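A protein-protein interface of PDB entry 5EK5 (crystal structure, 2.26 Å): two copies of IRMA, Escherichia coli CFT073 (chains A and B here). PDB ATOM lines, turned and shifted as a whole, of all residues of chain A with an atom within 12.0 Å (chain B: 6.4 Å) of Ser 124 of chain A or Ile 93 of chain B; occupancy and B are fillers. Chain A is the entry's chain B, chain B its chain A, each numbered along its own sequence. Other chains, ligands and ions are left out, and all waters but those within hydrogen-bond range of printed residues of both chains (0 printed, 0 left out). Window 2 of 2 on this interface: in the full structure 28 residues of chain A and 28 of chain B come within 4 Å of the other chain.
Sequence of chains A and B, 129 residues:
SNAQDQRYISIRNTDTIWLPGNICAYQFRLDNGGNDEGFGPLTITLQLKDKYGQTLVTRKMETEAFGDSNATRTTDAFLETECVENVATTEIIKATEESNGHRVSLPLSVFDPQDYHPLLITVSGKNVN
Ser 124 of chain A touches three residues of chain B.
Ile 93 of chain B touches just one residue of chain A: Ser 124.
Thr 45 of chain B touches none of the printed residues of chain A.
No residue of chain A comes within 4 Å of Leu 46 of chain B.
No residue of chain A comes within 4 Å of Gln 47 of chain B.
Ile 92 of chain B touches just these residues of chain A: Thr 122 (2.9 Å), Val 123 (3.7 Å) and Ser 124 (2.9 Å).
No residue of chain A comes within 4 Å of Ala 95 of chain B.
Of chain A, only Val 123 comes within 4 Å of Leu 108 of chain B.
Of the printed residues of chain B, Thr 122 of chain A touches Glu 91 and Ile 92.
Of the printed residues of chain B, Val 123 of chain A touches Ile 92 and Leu 108.
The nearest residue of chain B that does not touch Ser 124 of chain A is Leu 108 of chain B (4.03 Å).
The nearest residue of chain A that does not touch Ile 93 of chain B is Thr 122 of chain A (5.9 Å).
The nearest printed residue of chain B that does not touch Thr 122 of chain A is Ile 93 of chain B (5.9 Å).
Among the printed residues, merely in contact across the chains: Val 123 of chain A with Ile 92 of chain B, Val 123 of chain A with Leu 108 of chain B, Ser 124 of chain A with Glu 91 of chain B and Ser 124 of chain A with Ile 93 of chain B.
Of the 6 printed residues of chain A, 3 touch a printed residue of chain B.
Printed residues of chain A that touch a printed residue of chain B: Thr 122, Val 123 and Ser 124.
Of the 11 printed residues of chain B, 4 touch a printed residue of chain A.
Hydrophobic or aromatic side chains of chain B that line the printed part of chain A: Ile 92 and Leu 108.
Among the printed residues, no Asp or Glu carboxylate lies within 4 Å of a Lys or Arg side-chain nitrogen of the other chain.
No position is printed for both chains.
The side-chain carboxylate of Glu 91 of chain B is in hydrogen-bond range of the side-chain hydroxyl of Thr 122 of chain A.
The backbone carbonyl oxygen of Thr 122 of chain A is in hydrogen-bond range of the backbone NH of Ile 92 of chain B, 2.9 Å away.
O of Ile 92 of chain B lies within hydrogen-bond range of N of Ser 124 of chain A, at 2.9 Å.
N of Ile 93 of chain B is in hydrogen-bond range of O of Thr 45 of chain B, 3.1 Å away.
The backbone NH of Gln 47 of chain B is in hydrogen-bond range of the backbone carbonyl oxygen of Glu 91 of chain B (2.9 Å).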
ATOM      1  N   LEU A 120      12.811  19.042 -34.446  1.00  0.00           N
ATOM      2  CA  LEU A 120      13.444  18.806 -33.166  1.00  0.00           C
ATOM      3  C   LEU A 120      12.438  18.055 -32.304  1.00  0.00           C
ATOM      4  O   LEU A 120      11.238  18.323 -32.364  1.00  0.00           O
ATOM      5  CB  LEU A 120      13.881  20.120 -32.517  1.00  0.00           C
ATOM      6  CG  LEU A 120      14.825  20.002 -31.321  1.00  0.00           C
ATOM      7  CD1 LEU A 120      15.886  21.087 -31.370  1.00  0.00           C
ATOM      8  CD2 LEU A 120      14.034  20.096 -30.029  1.00  0.00           C
ATOM      9  N   ILE A 121      12.921  17.104 -31.517  1.00  0.00           N
ATOM     10  CA  ILE A 121      12.035  16.308 -30.683  1.00  0.00           C
ATOM     11  C   ILE A 121      12.376  16.466 -29.211  1.00  0.00           C
ATOM     12  O   ILE A 121      13.528  16.311 -28.807  1.00  0.00           O
ATOM     13  CB  ILE A 121      12.095  14.816 -31.060  1.00  0.00           C
ATOM     14  CG1 ILE A 121      11.778  14.631 -32.544  1.00  0.00           C
ATOM     15  CG2 ILE A 121      11.130  14.011 -30.203  1.00  0.00           C
ATOM     16  CD1 ILE A 121      11.957  13.213 -33.035  1.00  0.00           C
ATOM     17  N   THR A 122      11.363  16.800 -28.420  1.00  0.00           N
ATOM     18  CA  THR A 122      11.490  16.880 -26.974  1.00  0.00           C
ATOM     19  C   THR A 122      10.514  15.919 -26.311  1.00  0.00           C
ATOM     20  O   THR A 122       9.626  15.372 -26.966  1.00  0.00           O
ATOM     21  CB  THR A 122      11.225  18.300 -26.454  1.00  0.00           C
ATOM     22  OG1 THR A 122       9.911  18.716 -26.848  1.00  0.00           O
ATOM     23  CG2 THR A 122      12.249  19.273 -27.013  1.00  0.00           C
ATOM     24  N   VAL A 123      10.669  15.737 -25.006  1.00  0.00           N
ATOM     25  CA  VAL A 123       9.798  14.849 -24.252  1.00  0.00           C
ATOM     26  C   VAL A 123       9.234  15.586 -23.043  1.00  0.00           C
ATOM     27  O   VAL A 123       9.974  16.210 -22.286  1.00  0.00           O
ATOM     28  CB  VAL A 123      10.541  13.579 -23.790  1.00  0.00           C
ATOM     29  CG1 VAL A 123       9.684  12.779 -22.833  1.00  0.00           C
ATOM     30  CG2 VAL A 123      10.937  12.732 -24.987  1.00  0.00           C
ATOM     31  N   SER A 124       7.916  15.516 -22.880  1.00  0.00           N
ATOM     32  CA  SER A 124       7.221  16.245 -21.824  1.00  0.00           C
ATOM     33  C   SER A 124       7.580  15.753 -20.426  1.00  0.00           C
ATOM     34  O   SER A 124       8.014  14.616 -20.246  1.00  0.00           O
ATOM     35  CB  SER A 124       5.709  16.148 -22.024  1.00  0.00           C
ATOM     36  OG  SER A 124       5.020  16.528 -20.846  1.00  0.00           O
ATOM     37  N   GLY A 125       7.386  16.623 -19.440  1.00  0.00           N
ATOM     38  CA  GLY A 125       7.643  16.286 -18.051  1.00  0.00           C
ATOM     39  C   GLY A 125       6.384  16.304 -17.204  1.00  0.00           C
ATOM     40  O   GLY A 125       5.486  17.120 -17.417  1.00  0.00           O
ATOM     41  N   ILE B  44       2.056   6.825 -30.187  1.00  0.00           N
ATOM     42  CA  ILE B  44       2.759   7.965 -29.626  1.00  0.00           C
ATOM     43  C   ILE B  44       2.005   9.243 -29.938  1.00  0.00           C
ATOM     44  O   ILE B  44       1.663   9.506 -31.090  1.00  0.00           O
ATOM     45  CB  ILE B  44       4.194   8.064 -30.173  1.00  0.00           C
ATOM     46  CG1 ILE B  44       4.922   6.731 -29.983  1.00  0.00           C
ATOM     47  CG2 ILE B  44       4.949   9.212 -29.509  1.00  0.00           C
ATOM     48  CD1 ILE B  44       6.309   6.703 -30.581  1.00  0.00           C
ATOM     49  N   THR B  45       1.742  10.033 -28.905  1.00  0.00           N
ATOM     50  CA  THR B  45       1.028  11.286 -29.078  1.00  0.00           C
ATOM     51  C   THR B  45       2.025  12.435 -29.160  1.00  0.00           C
ATOM     52  O   THR B  45       2.841  12.630 -28.258  1.00  0.00           O
ATOM     53  CB  THR B  45       0.037  11.543 -27.930  1.00  0.00           C
ATOM     54  OG1 THR B  45      -0.877  10.442 -27.828  1.00  0.00           O
ATOM     55  CG2 THR B  45      -0.743  12.821 -28.181  1.00  0.00           C
ATOM     56  N   LEU B  46       1.960  13.185 -30.256  1.00  0.00           N
ATOM     57  CA  LEU B  46       2.907  14.268 -30.491  1.00  0.00           C
ATOM     58  C   LEU B  46       2.218  15.620 -30.553  1.00  0.00           C
ATOM     59  O   LEU B  46       1.197  15.783 -31.221  1.00  0.00           O
ATOM     60  CB  LEU B  46       3.685  14.055 -31.799  1.00  0.00           C
ATOM     61  CG  LEU B  46       4.642  12.876 -32.011  1.00  0.00           C
ATOM     62  CD1 LEU B  46       5.645  12.787 -30.876  1.00  0.00           C
ATOM     63  CD2 LEU B  46       3.907  11.557 -32.200  1.00  0.00           C
ATOM     64  N   GLN B  47       2.789  16.592 -29.854  1.00  0.00           N
ATOM     65  CA  GLN B  47       2.421  17.979 -30.063  1.00  0.00           C
ATOM     66  C   GLN B  47       3.292  18.552 -31.165  1.00  0.00           C
ATOM     67  O   GLN B  47       4.511  18.593 -31.032  1.00  0.00           O
ATOM     68  CB  GLN B  47       2.592  18.794 -28.784  1.00  0.00           C
ATOM     69  CG  GLN B  47       1.451  18.660 -27.801  1.00  0.00           C
ATOM     70  CD  GLN B  47       1.683  19.466 -26.544  1.00  0.00           C
ATOM     71  OE1 GLN B  47       2.818  19.810 -26.215  1.00  0.00           O
ATOM     72  NE2 GLN B  47       0.608  19.763 -25.824  1.00  0.00           N
ATOM     73  N   THR B  58      -2.249  18.459 -32.270  1.00  0.00           N
ATOM     74  CA  THR B  58      -1.810  17.283 -31.537  1.00  0.00           C
ATOM     75  C   THR B  58      -2.220  16.042 -32.316  1.00  0.00           C
ATOM     76  O   THR B  58      -3.387  15.876 -32.663  1.00  0.00           O
ATOM     77  CB  THR B  58      -2.408  17.247 -30.120  1.00  0.00           C
ATOM     78  OG1 THR B  58      -1.954  18.388 -29.384  1.00  0.00           O
ATOM     79  CG2 THR B  58      -1.996  15.982 -29.391  1.00  0.00           C
ATOM     80  N   GLU B  91       6.833  17.582 -29.590  1.00  0.00           N
ATOM     81  CA  GLU B  91       7.024  17.100 -28.226  1.00  0.00           C
ATOM     82  C   GLU B  91       6.183  15.866 -27.915  1.00  0.00           C
ATOM     83  O   GLU B  91       4.967  15.864 -28.101  1.00  0.00           O
ATOM     84  CB  GLU B  91       6.707  18.201 -27.212  1.00  0.00           C
ATOM     85  CG  GLU B  91       6.735  17.721 -25.767  1.00  0.00           C
ATOM     86  CD  GLU B  91       6.820  18.857 -24.768  1.00  0.00           C
ATOM     87  OE1 GLU B  91       7.796  19.634 -24.836  1.00  0.00           O
ATOM     88  OE2 GLU B  91       5.913  18.971 -23.914  1.00  0.00           O
ATOM     89  N   ILE B  92       6.848  14.818 -27.442  1.00  0.00           N
ATOM     90  CA  ILE B  92       6.178  13.598 -27.014  1.00  0.00           C
ATOM     91  C   ILE B  92       5.506  13.819 -25.662  1.00  0.00           C
ATOM     92  O   ILE B  92       6.175  14.108 -24.668  1.00  0.00           O
ATOM     93  CB  ILE B  92       7.168  12.419 -26.904  1.00  0.00           C
ATOM     94  CG1 ILE B  92       7.895  12.200 -28.237  1.00  0.00           C
ATOM     95  CG2 ILE B  92       6.451  11.157 -26.455  1.00  0.00           C
ATOM     96  CD1 ILE B  92       8.992  11.154 -28.188  1.00  0.00           C
ATOM     97  N   ILE B  93       4.185  13.684 -25.622  1.00  0.00           N
ATOM     98  CA  ILE B  93       3.445  13.931 -24.392  1.00  0.00           C
ATOM     99  C   ILE B  93       2.801  12.652 -23.859  1.00  0.00           C
ATOM    100  O   ILE B  93       2.396  12.589 -22.699  1.00  0.00           O
ATOM    101  CB  ILE B  93       2.364  15.017 -24.597  1.00  0.00           C
ATOM    102  CG1 ILE B  93       1.306  14.563 -25.604  1.00  0.00           C
ATOM    103  CG2 ILE B  93       3.003  16.326 -25.048  1.00  0.00           C
ATOM    104  CD1 ILE B  93       0.125  15.512 -25.705  1.00  0.00           C
ATOM    105  N   LYS B  94       2.721  11.630 -24.704  1.00  0.00           N
ATOM    106  CA  LYS B  94       2.180  10.338 -24.292  1.00  0.00           C
ATOM    107  C   LYS B  94       2.659   9.207 -25.195  1.00  0.00           C
ATOM    108  O   LYS B  94       2.901   9.411 -26.383  1.00  0.00           O
ATOM    109  CB  LYS B  94       0.646  10.360 -24.293  1.00  0.00           C
ATOM    110  CG  LYS B  94       0.012   9.134 -23.645  1.00  0.00           C
ATOM    111  CD  LYS B  94      -1.455   9.344 -23.320  1.00  0.00           C
ATOM    112  CE  LYS B  94      -2.283   9.377 -24.596  1.00  0.00           C
ATOM    113  NZ  LYS B  94      -3.746   9.362 -24.323  1.00  0.00           N
ATOM    114  N   ALA B  95       2.776   8.010 -24.628  1.00  0.00           N
ATOM    115  CA  ALA B  95       3.118   6.827 -25.405  1.00  0.00           C
ATOM    116  C   ALA B  95       2.431   5.598 -24.822  1.00  0.00           C
ATOM    117  O   ALA B  95       2.437   5.380 -23.611  1.00  0.00           O
ATOM    118  CB  ALA B  95       4.621   6.626 -25.443  1.00  0.00           C
ATOM    119  N   LEU B 108       7.730   8.003 -20.380  1.00  0.00           N
ATOM    120  CA  LEU B 108       8.322   8.859 -21.400  1.00  0.00           C
ATOM    121  C   LEU B 108       9.835   8.979 -21.243  1.00  0.00           C
ATOM    122  O   LEU B 108      10.530   9.401 -22.167  1.00  0.00           O
ATOM    123  CB  LEU B 108       7.678  10.245 -21.362  1.00  0.00           C
ATOM    124  CG  LEU B 108       6.171  10.306 -21.620  1.00  0.00           C
ATOM    125  CD1 LEU B 108       5.742  11.735 -21.913  1.00  0.00           C
ATOM    126  CD2 LEU B 108       5.775   9.377 -22.762  1.00  0.00           C
